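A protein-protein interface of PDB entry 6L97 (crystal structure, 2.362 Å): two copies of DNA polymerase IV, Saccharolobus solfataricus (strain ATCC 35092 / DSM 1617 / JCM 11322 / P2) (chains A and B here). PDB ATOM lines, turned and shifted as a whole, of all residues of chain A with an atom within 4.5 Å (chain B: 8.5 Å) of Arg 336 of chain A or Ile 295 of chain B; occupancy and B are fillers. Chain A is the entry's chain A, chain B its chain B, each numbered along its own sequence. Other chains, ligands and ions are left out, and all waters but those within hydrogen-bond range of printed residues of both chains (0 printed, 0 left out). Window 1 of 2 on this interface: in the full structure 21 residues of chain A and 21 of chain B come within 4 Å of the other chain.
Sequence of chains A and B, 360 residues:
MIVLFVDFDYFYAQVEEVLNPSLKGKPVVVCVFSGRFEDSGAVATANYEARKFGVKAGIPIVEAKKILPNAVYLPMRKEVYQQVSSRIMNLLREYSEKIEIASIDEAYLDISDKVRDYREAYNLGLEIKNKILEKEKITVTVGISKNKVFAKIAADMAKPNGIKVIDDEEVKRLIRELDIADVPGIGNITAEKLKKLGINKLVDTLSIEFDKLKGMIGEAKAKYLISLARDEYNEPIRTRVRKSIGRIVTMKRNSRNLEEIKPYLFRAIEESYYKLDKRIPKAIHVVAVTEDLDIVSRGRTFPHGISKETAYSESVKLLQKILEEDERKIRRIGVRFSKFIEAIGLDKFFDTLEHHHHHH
Of the printed residues of chain B, Ser 244 of chain A touches Ile 295 (3.5 Å).
Of the printed residues of chain B, Gly 246 of chain A touches Asp 294.
No residue of chain B comes within 4 Å of Val 335 of chain A.
Arg 336 of chain A touches two residues of chain B.
Printed residues of chain A within 4 Å of Asp 294 of chain B: Gly 246 (2.8 Å).
The nearest residue of chain B that does not touch Arg 336 of chain A is Val 296 of chain B (4.8 Å).
The guanidinium group (NH2) of Arg 336 of chain A lies within hydrogen-bond range of the side-chain hydroxyl (OG) of Ser 244 of chain A.
O of His 285 of chain A lies within hydrogen-bond range of N of Arg 336 of chain A, at 2.7 Å.
O of Arg 332 of chain B is in hydrogen-bond range of N of Val 289 of chain B (2.8 Å).
The side-chain hydroxyl (OG1) of Thr 290 of chain B sits at hydrogen-bond distance from the backbone NH (N) of Asp 294 of chain B (3.2 Å).
OD2 of Asp 294 of chain B lies within salt-bridge range of NH1 of Arg 328 of chain B, at 2.8 Å.
Among the printed residues, merely in contact across the chains: Ser 244 of chain A with Ile 295 of chain B (3.5 Å), Arg 336 of chain A with Ile 295 of chain B (3.6 Å), Arg 336 of chain A with Ser 297 of chain B (3.6 Å) and Ile 248 of chain A with Arg 332 of chain B (3.98 Å).
Of the 12 printed residues of chain A, 4 touch a printed residue of chain B.
Printed residues of chain A that touch a printed residue of chain B: Ser 244, Gly 246, Ile 248 and Arg 336.
Hydrophobic or aromatic side chains of chain A that line the printed part of chain B: Ile 248.
Printed residues of chain B that touch a printed residue of chain A: Leu 293, Asp 294, Ile 295, Ser 297 and Arg 332.
Hydrophobic or aromatic side chains of chain B within 4 Å of the printed part of chain A: Leu 293 and Ile 295.
Among the printed residues, 6 pairs touch across the chains.
The backbone NH of Gly 246 of chain A lies within hydrogen-bond range of the side-chain carboxylate of Asp 294 of chain B, at 3.1 Å.
N of Ile 248 of chain A is in hydrogen-bond range of O of Leu 293 of chain B (2.9 Å).
4 positions are printed for both chains.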
ATOM      1  N   SER A 244      30.236  -1.031   6.874  1.00  0.00           N
ATOM      2  CA  SER A 244      30.554   0.289   7.391  1.00  0.00           C
ATOM      3  C   SER A 244      30.982   0.161   8.844  1.00  0.00           C
ATOM      4  O   SER A 244      30.474  -0.692   9.575  1.00  0.00           O
ATOM      5  CB  SER A 244      29.359   1.249   7.261  1.00  0.00           C
ATOM      6  OG  SER A 244      28.603   1.309   8.460  1.00  0.00           O
ATOM      7  N   ILE A 245      31.930   1.005   9.252  1.00  0.00           N
ATOM      8  CA  ILE A 245      32.455   1.032  10.613  1.00  0.00           C
ATOM      9  C   ILE A 245      32.397   2.468  11.110  1.00  0.00           C
ATOM     10  O   ILE A 245      32.932   3.374  10.463  1.00  0.00           O
ATOM     11  CB  ILE A 245      33.900   0.497  10.683  1.00  0.00           C
ATOM     12  CG1 ILE A 245      33.923  -1.020  10.497  1.00  0.00           C
ATOM     13  CG2 ILE A 245      34.556   0.882  12.009  1.00  0.00           C
ATOM     14  CD1 ILE A 245      33.604  -1.794  11.756  1.00  0.00           C
ATOM     15  N   GLY A 246      31.753   2.679  12.251  1.00  0.00           N
ATOM     16  CA  GLY A 246      31.628   4.022  12.765  1.00  0.00           C
ATOM     17  C   GLY A 246      31.261   4.041  14.232  1.00  0.00           C
ATOM     18  O   GLY A 246      31.298   3.019  14.920  1.00  0.00           O
ATOM     19  N   ILE A 248      28.763   6.761  17.046  1.00  0.00           N
ATOM     20  CA  ILE A 248      28.025   7.977  17.366  1.00  0.00           C
ATOM     21  C   ILE A 248      28.092   8.199  18.871  1.00  0.00           C
ATOM     22  O   ILE A 248      27.883   7.266  19.654  1.00  0.00           O
ATOM     23  CB  ILE A 248      26.565   7.907  16.877  1.00  0.00           C
ATOM     24  CG1 ILE A 248      25.820   9.185  17.249  1.00  0.00           C
ATOM     25  CG2 ILE A 248      25.849   6.684  17.432  1.00  0.00           C
ATOM     26  CD1 ILE A 248      24.859   9.622  16.188  1.00  0.00           C
ATOM     27  N   ALA A 283      35.383   6.325   1.878  1.00  0.00           N
ATOM     28  CA  ALA A 283      34.261   7.218   2.145  1.00  0.00           C
ATOM     29  C   ALA A 283      34.190   7.535   3.630  1.00  0.00           C
ATOM     30  O   ALA A 283      34.326   6.635   4.467  1.00  0.00           O
ATOM     31  CB  ALA A 283      32.933   6.610   1.678  1.00  0.00           C
ATOM     32  N   ILE A 284      33.983   8.813   3.954  1.00  0.00           N
ATOM     33  CA  ILE A 284      33.706   9.257   5.317  1.00  0.00           C
ATOM     34  C   ILE A 284      32.349   9.951   5.320  1.00  0.00           C
ATOM     35  O   ILE A 284      32.012  10.682   4.382  1.00  0.00           O
ATOM     36  CB  ILE A 284      34.813  10.188   5.866  1.00  0.00           C
ATOM     37  CG1 ILE A 284      34.535  10.561   7.321  1.00  0.00           C
ATOM     38  CG2 ILE A 284      34.947  11.459   5.029  1.00  0.00           C
ATOM     39  CD1 ILE A 284      35.536  11.547   7.894  1.00  0.00           C
ATOM     40  N   HIS A 285      31.554   9.689   6.356  1.00  0.00           N
ATOM     41  CA  HIS A 285      30.235  10.292   6.517  1.00  0.00           C
ATOM     42  C   HIS A 285      30.122  10.822   7.937  1.00  0.00           C
ATOM     43  O   HIS A 285      30.381  10.088   8.895  1.00  0.00           O
ATOM     44  CB  HIS A 285      29.112   9.281   6.249  1.00  0.00           C
ATOM     45  CG  HIS A 285      28.760   9.119   4.802  1.00  0.00           C
ATOM     46  ND1 HIS A 285      27.693   9.768   4.220  1.00  0.00           N
ATOM     47  CD2 HIS A 285      29.319   8.366   3.825  1.00  0.00           C
ATOM     48  CE1 HIS A 285      27.616   9.429   2.945  1.00  0.00           C
ATOM     49  NE2 HIS A 285      28.592   8.579   2.680  1.00  0.00           N
ATOM     50  N   VAL A 287      27.600  12.191  10.802  1.00  0.00           N
ATOM     51  CA  VAL A 287      26.204  11.918  11.128  1.00  0.00           C
ATOM     52  C   VAL A 287      25.845  12.744  12.350  1.00  0.00           C
ATOM     53  O   VAL A 287      26.483  12.611  13.403  1.00  0.00           O
ATOM     54  CB  VAL A 287      25.960  10.424  11.407  1.00  0.00           C
ATOM     55  CG1 VAL A 287      24.484  10.168  11.705  1.00  0.00           C
ATOM     56  CG2 VAL A 287      26.438   9.583  10.251  1.00  0.00           C
ATOM     57  N   VAL A 335      30.597   9.566  13.140  1.00  0.00           N
ATOM     58  CA  VAL A 335      31.270   9.408  11.859  1.00  0.00           C
ATOM     59  C   VAL A 335      31.045   7.978  11.386  1.00  0.00           C
ATOM     60  O   VAL A 335      30.859   7.065  12.195  1.00  0.00           O
ATOM     61  CB  VAL A 335      32.774   9.733  11.987  1.00  0.00           C
ATOM     62  CG1 VAL A 335      33.398   8.882  13.078  1.00  0.00           C
ATOM     63  CG2 VAL A 335      33.503   9.573  10.657  1.00  0.00           C
ATOM     64  N   ARG A 336      31.036   7.787  10.067  1.00  0.00           N
ATOM     65  CA  ARG A 336      30.865   6.468   9.466  1.00  0.00           C
ATOM     66  C   ARG A 336      31.866   6.291   8.336  1.00  0.00           C
ATOM     67  O   ARG A 336      31.938   7.128   7.431  1.00  0.00           O
ATOM     68  CB  ARG A 336      29.449   6.275   8.918  1.00  0.00           C
ATOM     69  CG  ARG A 336      28.390   6.048   9.967  1.00  0.00           C
ATOM     70  CD  ARG A 336      27.036   5.892   9.310  1.00  0.00           C
ATOM     71  NE  ARG A 336      26.912   4.615   8.614  1.00  0.00           N
ATOM     72  CZ  ARG A 336      25.860   4.263   7.882  1.00  0.00           C
ATOM     73  NH1 ARG A 336      24.833   5.093   7.747  1.00  0.00           N
ATOM     74  NH2 ARG A 336      25.831   3.079   7.288  1.00  0.00           N
ATOM     75  N   PHE A 337      32.613   5.191   8.374  1.00  0.00           N
ATOM     76  CA  PHE A 337      33.583   4.865   7.338  1.00  0.00           C
ATOM     77  C   PHE A 337      33.093   3.694   6.500  1.00  0.00           C
ATOM     78  O   PHE A 337      32.534   2.729   7.029  1.00  0.00           O
ATOM     79  CB  PHE A 337      34.935   4.532   7.952  1.00  0.00           C
ATOM     80  CG  PHE A 337      35.616   5.709   8.562  1.00  0.00           C
ATOM     81  CD1 PHE A 337      36.050   6.761   7.768  1.00  0.00           C
ATOM     82  CD2 PHE A 337      35.806   5.778   9.934  1.00  0.00           C
ATOM     83  CE1 PHE A 337      36.679   7.851   8.328  1.00  0.00           C
ATOM     84  CE2 PHE A 337      36.432   6.874  10.503  1.00  0.00           C
ATOM     85  CZ  PHE A 337      36.869   7.911   9.697  1.00  0.00           C
ATOM     86  N   SER A 338      33.311   3.781   5.190  1.00  0.00           N
ATOM     87  CA  SER A 338      32.844   2.758   4.265  1.00  0.00           C
ATOM     88  C   SER A 338      33.766   2.726   3.051  1.00  0.00           C
ATOM     89  O   SER A 338      34.688   3.536   2.924  1.00  0.00           O
ATOM     90  CB  SER A 338      31.395   3.020   3.858  1.00  0.00           C
ATOM     91  OG  SER A 338      31.282   4.268   3.193  1.00  0.00           O
ATOM     92  N   ILE B 248      14.897   8.940  15.239  1.00  0.00           N
ATOM     93  CA  ILE B 248      15.535   7.783  15.856  1.00  0.00           C
ATOM     94  C   ILE B 248      15.107   7.726  17.316  1.00  0.00           C
ATOM     95  O   ILE B 248      15.154   8.738  18.023  1.00  0.00           O
ATOM     96  CB  ILE B 248      17.070   7.820  15.704  1.00  0.00           C
ATOM     97  CG1 ILE B 248      17.696   6.568  16.316  1.00  0.00           C
ATOM     98  CG2 ILE B 248      17.674   9.076  16.306  1.00  0.00           C
ATOM     99  CD1 ILE B 248      18.775   5.977  15.453  1.00  0.00           C
ATOM    100  N   HIS B 285      15.085   4.578   4.668  1.00  0.00           N
ATOM    101  CA  HIS B 285      16.278   4.013   5.277  1.00  0.00           C
ATOM    102  C   HIS B 285      15.970   3.661   6.721  1.00  0.00           C
ATOM    103  O   HIS B 285      15.431   4.485   7.463  1.00  0.00           O
ATOM    104  CB  HIS B 285      17.455   4.987   5.192  1.00  0.00           C
ATOM    105  CG  HIS B 285      18.055   5.076   3.825  1.00  0.00           C
ATOM    106  ND1 HIS B 285      19.190   4.382   3.464  1.00  0.00           N
ATOM    107  CD2 HIS B 285      17.666   5.758   2.722  1.00  0.00           C
ATOM    108  CE1 HIS B 285      19.475   4.634   2.200  1.00  0.00           C
ATOM    109  NE2 HIS B 285      18.568   5.469   1.728  1.00  0.00           N
ATOM    110  N   VAL B 286      16.284   2.434   7.106  1.00  0.00           N
ATOM    111  CA  VAL B 286      16.201   2.022   8.500  1.00  0.00           C
ATOM    112  C   VAL B 286      17.591   2.146   9.100  1.00  0.00           C
ATOM    113  O   VAL B 286      18.573   1.657   8.529  1.00  0.00           O
ATOM    114  CB  VAL B 286      15.649   0.594   8.628  1.00  0.00           C
ATOM    115  CG1 VAL B 286      15.902   0.044  10.022  1.00  0.00           C
ATOM    116  CG2 VAL B 286      14.156   0.588   8.332  1.00  0.00           C
ATOM    117  N   VAL B 287      17.677   2.840  10.229  1.00  0.00           N
ATOM    118  CA  VAL B 287      18.935   3.142  10.891  1.00  0.00           C
ATOM    119  C   VAL B 287      18.917   2.473  12.251  1.00  0.00           C
ATOM    120  O   VAL B 287      17.982   2.673  13.033  1.00  0.00           O
ATOM    121  CB  VAL B 287      19.152   4.660  11.038  1.00  0.00           C
ATOM    122  CG1 VAL B 287      20.569   4.943  11.519  1.00  0.00           C
ATOM    123  CG2 VAL B 287      18.882   5.368   9.722  1.00  0.00           C
ATOM    124  N   ALA B 288      19.948   1.689  12.533  1.00  0.00           N
ATOM    125  CA  ALA B 288      20.055   0.955  13.783  1.00  0.00           C
ATOM    126  C   ALA B 288      21.331   1.371  14.494  1.00  0.00           C
ATOM    127  O   ALA B 288      22.409   1.380  13.892  1.00  0.00           O
ATOM    128  CB  ALA B 288      20.049  -0.555  13.537  1.00  0.00           C
ATOM    129  N   VAL B 289      21.205   1.721  15.767  1.00  0.00           N
ATOM    130  CA  VAL B 289      22.350   2.072  16.596  1.00  0.00           C
ATOM    131  C   VAL B 289      22.612   0.891  17.522  1.00  0.00           C
ATOM    132  O   VAL B 289      21.796   0.577  18.395  1.00  0.00           O
ATOM    133  CB  VAL B 289      22.113   3.374  17.371  1.00  0.00           C
ATOM    134  CG1 VAL B 289      23.265   3.646  18.311  1.00  0.00           C
ATOM    135  CG2 VAL B 289      21.949   4.530  16.394  1.00  0.00           C
ATOM    136  N   THR B 290      23.744   0.225  17.319  1.00  0.00           N
ATOM    137  CA  THR B 290      24.054  -1.004  18.029  1.00  0.00           C
ATOM    138  C   THR B 290      24.498  -0.700  19.460  1.00  0.00           C
ATOM    139  O   THR B 290      24.588   0.458  19.881  1.00  0.00           O
ATOM    140  CB  THR B 290      25.117  -1.794  17.268  1.00  0.00           C
ATOM    141  OG1 THR B 290      26.281  -0.979  17.088  1.00  0.00           O
ATOM    142  CG2 THR B 290      24.588  -2.196  15.903  1.00  0.00           C
ATOM    143  N   GLU B 291      24.782  -1.765  20.217  1.00  0.00           N
ATOM    144  CA  GLU B 291      25.098  -1.614  21.637  1.00  0.00           C
ATOM    145  C   GLU B 291      26.385  -0.826  21.847  1.00  0.00           C
ATOM    146  O   GLU B 291      26.487  -0.028  22.787  1.00  0.00           O
ATOM    147  CB  GLU B 291      25.199  -2.988  22.302  1.00  0.00           C
ATOM    148  CG  GLU B 291      25.589  -2.932  23.774  1.00  0.00           C
ATOM    149  CD  GLU B 291      25.218  -4.194  24.532  1.00  0.00           C
ATOM    150  OE1 GLU B 291      24.637  -4.077  25.632  1.00  0.00           O
ATOM    151  OE2 GLU B 291      25.512  -5.300  24.031  1.00  0.00           O
ATOM    152  N   ASP B 292      27.384  -1.041  20.988  1.00  0.00           N
ATOM    153  CA  ASP B 292      28.610  -0.251  21.002  1.00  0.00           C
ATOM    154  C   ASP B 292      28.444   1.101  20.322  1.00  0.00           C
ATOM    155  O   ASP B 292      29.451   1.728  19.971  1.00  0.00           O
ATOM    156  CB  ASP B 292      29.750  -1.031  20.342  1.00  0.00           C
ATOM    157  CG  ASP B 292      29.310  -1.749  19.083  1.00  0.00           C
ATOM    158  OD1 ASP B 292      28.108  -2.069  18.978  1.00  0.00           O
ATOM    159  OD2 ASP B 292      30.162  -1.997  18.202  1.00  0.00           O
ATOM    160  N   LEU B 293      27.201   1.547  20.126  1.00  0.00           N
ATOM    161  CA  LEU B 293      26.903   2.860  19.555  1.00  0.00           C
ATOM    162  C   LEU B 293      27.528   3.023  18.169  1.00  0.00           C
ATOM    163  O   LEU B 293      28.089   4.069  17.836  1.00  0.00           O
ATOM    164  CB  LEU B 293      27.337   3.980  20.503  1.00  0.00           C
ATOM    165  CG  LEU B 293      26.526   4.044  21.802  1.00  0.00           C
ATOM    166  CD1 LEU B 293      27.012   5.175  22.697  1.00  0.00           C
ATOM    167  CD2 LEU B 293      25.040   4.204  21.503  1.00  0.00           C
ATOM    168  N   ASP B 294      27.435   1.971  17.360  1.00  0.00           N
ATOM    169  CA  ASP B 294      27.761   2.010  15.943  1.00  0.00           C
ATOM    170  C   ASP B 294      26.470   2.132  15.136  1.00  0.00           C
ATOM    171  O   ASP B 294      25.383   1.798  15.612  1.00  0.00           O
ATOM    172  CB  ASP B 294      28.541   0.754  15.535  1.00  0.00           C
ATOM    173  CG  ASP B 294      29.163   0.867  14.149  1.00  0.00           C
ATOM    174  OD1 ASP B 294      29.066   1.948  13.537  1.00  0.00           O
ATOM    175  OD2 ASP B 294      29.761  -0.126  13.676  1.00  0.00           O
ATOM    176  N   ILE B 295      26.597   2.626  13.906  1.00  0.00           N
ATOM    177  CA  ILE B 295      25.449   2.872  13.037  1.00  0.00           C
ATOM    178  C   ILE B 295      25.442   1.828  11.932  1.00  0.00           C
ATOM    179  O   ILE B 295      26.417   1.697  11.180  1.00  0.00           O
ATOM    180  CB  ILE B 295      25.472   4.286  12.439  1.00  0.00           C
ATOM    181  CG1 ILE B 295      25.210   5.335  13.521  1.00  0.00           C
ATOM    182  CG2 ILE B 295      24.445   4.390  11.312  1.00  0.00           C
ATOM    183  CD1 ILE B 295      23.765   5.769  13.616  1.00  0.00           C
ATOM    184  N   VAL B 296      24.339   1.095  11.827  1.00  0.00           N
ATOM    185  CA  VAL B 296      24.102   0.152  10.743  1.00  0.00           C
ATOM    186  C   VAL B 296      22.829   0.583  10.033  1.00  0.00           C
ATOM    187  O   VAL B 296      21.807   0.833  10.683  1.00  0.00           O
ATOM    188  CB  VAL B 296      23.988  -1.293  11.260  1.00  0.00           C
ATOM    189  CG1 VAL B 296      23.964  -2.265  10.102  1.00  0.00           C
ATOM    190  CG2 VAL B 296      25.139  -1.609  12.203  1.00  0.00           C
ATOM    191  N   SER B 297      22.886   0.672   8.707  1.00  0.00           N
ATOM    192  CA  SER B 297      21.796   1.258   7.945  1.00  0.00           C
ATOM    193  C   SER B 297      21.589   0.508   6.636  1.00  0.00           C
ATOM    194  O   SER B 297      22.552   0.077   5.996  1.00  0.00           O
ATOM    195  CB  SER B 297      22.068   2.738   7.666  1.00  0.00           C
ATOM    196  OG  SER B 297      21.537   3.120   6.413  1.00  0.00           O
ATOM    197  N   ARG B 298      20.323   0.361   6.250  1.00  0.00           N
ATOM    198  CA  ARG B 298      19.936  -0.249   4.987  1.00  0.00           C
ATOM    199  C   ARG B 298      18.734   0.501   4.436  1.00  0.00           C
ATOM    200  O   ARG B 298      17.836   0.888   5.190  1.00  0.00           O
ATOM    201  CB  ARG B 298      19.592  -1.731   5.154  1.00  0.00           C
ATOM    202  CG  ARG B 298      20.735  -2.596   5.643  1.00  0.00           C
ATOM    203  CD  ARG B 298      21.784  -2.800   4.574  1.00  0.00           C
ATOM    204  NE  ARG B 298      22.870  -3.647   5.059  1.00  0.00           N
ATOM    205  CZ  ARG B 298      23.913  -3.199   5.752  1.00  0.00           C
ATOM    206  NH1 ARG B 298      24.013  -1.907   6.041  1.00  0.00           N
ATOM    207  NH2 ARG B 298      24.855  -4.043   6.155  1.00  0.00           N
ATOM    208  N   ILE B 322      19.076  -6.002   8.657  1.00  0.00           N
ATOM    209  CA  ILE B 322      20.053  -5.526   9.591  1.00  0.00           C
ATOM    210  C   ILE B 322      20.316  -6.645  10.587  1.00  0.00           C
ATOM    211  O   ILE B 322      21.446  -7.026  10.777  1.00  0.00           O
ATOM    212  CB  ILE B 322      19.612  -4.222  10.251  1.00  0.00           C
ATOM    213  CG1 ILE B 322      19.707  -3.101   9.217  1.00  0.00           C
ATOM    214  CG2 ILE B 322      20.437  -3.923  11.490  1.00  0.00           C
ATOM    215  CD1 ILE B 322      18.910  -1.867   9.521  1.00  0.00           C
ATOM    216  N   ASP B 326      24.206  -8.341  11.129  1.00  0.00           N
ATOM    217  CA  ASP B 326      24.956  -7.770  12.240  1.00  0.00           C
ATOM    218  C   ASP B 326      24.590  -8.499  13.524  1.00  0.00           C
ATOM    219  O   ASP B 326      23.407  -8.700  13.812  1.00  0.00           O
ATOM    220  CB  ASP B 326      24.690  -6.269  12.380  1.00  0.00           C
ATOM    221  CG  ASP B 326      25.899  -5.515  12.898  1.00  0.00           C
ATOM    222  OD1 ASP B 326      26.262  -5.712  14.076  1.00  0.00           O
ATOM    223  OD2 ASP B 326      26.494  -4.734  12.125  1.00  0.00           O
ATOM    224  N   ARG B 328      25.560  -7.625  16.729  1.00  0.00           N
ATOM    225  CA  ARG B 328      25.508  -6.820  17.936  1.00  0.00           C
ATOM    226  C   ARG B 328      24.061  -6.526  18.327  1.00  0.00           C
ATOM    227  O   ARG B 328      23.146  -6.545  17.499  1.00  0.00           O
ATOM    228  CB  ARG B 328      26.287  -5.517  17.743  1.00  0.00           C
ATOM    229  CG  ARG B 328      27.666  -5.710  17.113  1.00  0.00           C
ATOM    230  CD  ARG B 328      28.315  -4.380  16.745  1.00  0.00           C
ATOM    231  NE  ARG B 328      27.959  -3.957  15.394  1.00  0.00           N
ATOM    232  CZ  ARG B 328      28.634  -3.058  14.684  1.00  0.00           C
ATOM    233  NH1 ARG B 328      29.710  -2.472  15.193  1.00  0.00           N
ATOM    234  NH2 ARG B 328      28.227  -2.741  13.463  1.00  0.00           N
ATOM    235  N   ARG B 332      19.178   1.643  19.677  1.00  0.00           N
ATOM    236  CA  ARG B 332      18.221   2.599  19.149  1.00  0.00           C
ATOM    237  C   ARG B 332      17.877   2.205  17.718  1.00  0.00           C
ATOM    238  O   ARG B 332      18.698   1.618  17.008  1.00  0.00           O
ATOM    239  CB  ARG B 332      18.783   4.035  19.198  1.00  0.00           C
ATOM    240  CG  ARG B 332      19.663   4.323  20.417  1.00  0.00           C
ATOM    241  CD  ARG B 332      19.775   5.815  20.689  1.00  0.00           C
ATOM    242  NE  ARG B 332      21.033   6.360  20.195  1.00  0.00           N
ATOM    243  CZ  ARG B 332      22.119   6.536  20.941  1.00  0.00           C
ATOM    244  NH1 ARG B 332      22.101   6.216  22.225  1.00  0.00           N
ATOM    245  NH2 ARG B 332      23.223   7.034  20.400  1.00  0.00           N
ATOM    246  N   ARG B 336      14.372   7.127   8.279  1.00  0.00           N
ATOM    247  CA  ARG B 336      14.509   8.426   7.635  1.00  0.00           C
ATOM    248  C   ARG B 336      13.991   8.323   6.208  1.00  0.00           C
ATOM    249  O   ARG B 336      14.104   7.278   5.562  1.00  0.00           O
ATOM    250  CB  ARG B 336      15.959   8.922   7.649  1.00  0.00           C
ATOM    251  CG  ARG B 336      16.849   8.315   6.599  1.00  0.00           C
ATOM    252  CD  ARG B 336      18.248   8.892   6.706  1.00  0.00           C
ATOM    253  NE  ARG B 336      19.084   8.542   5.560  1.00  0.00           N
ATOM    254  CZ  ARG B 336      19.251   9.316   4.494  1.00  0.00           C
ATOM    255  NH1 ARG B 336      18.633  10.490   4.418  1.00  0.00           N
ATOM    256  NH2 ARG B 336      20.035   8.912   3.501  1.00  0.00           N
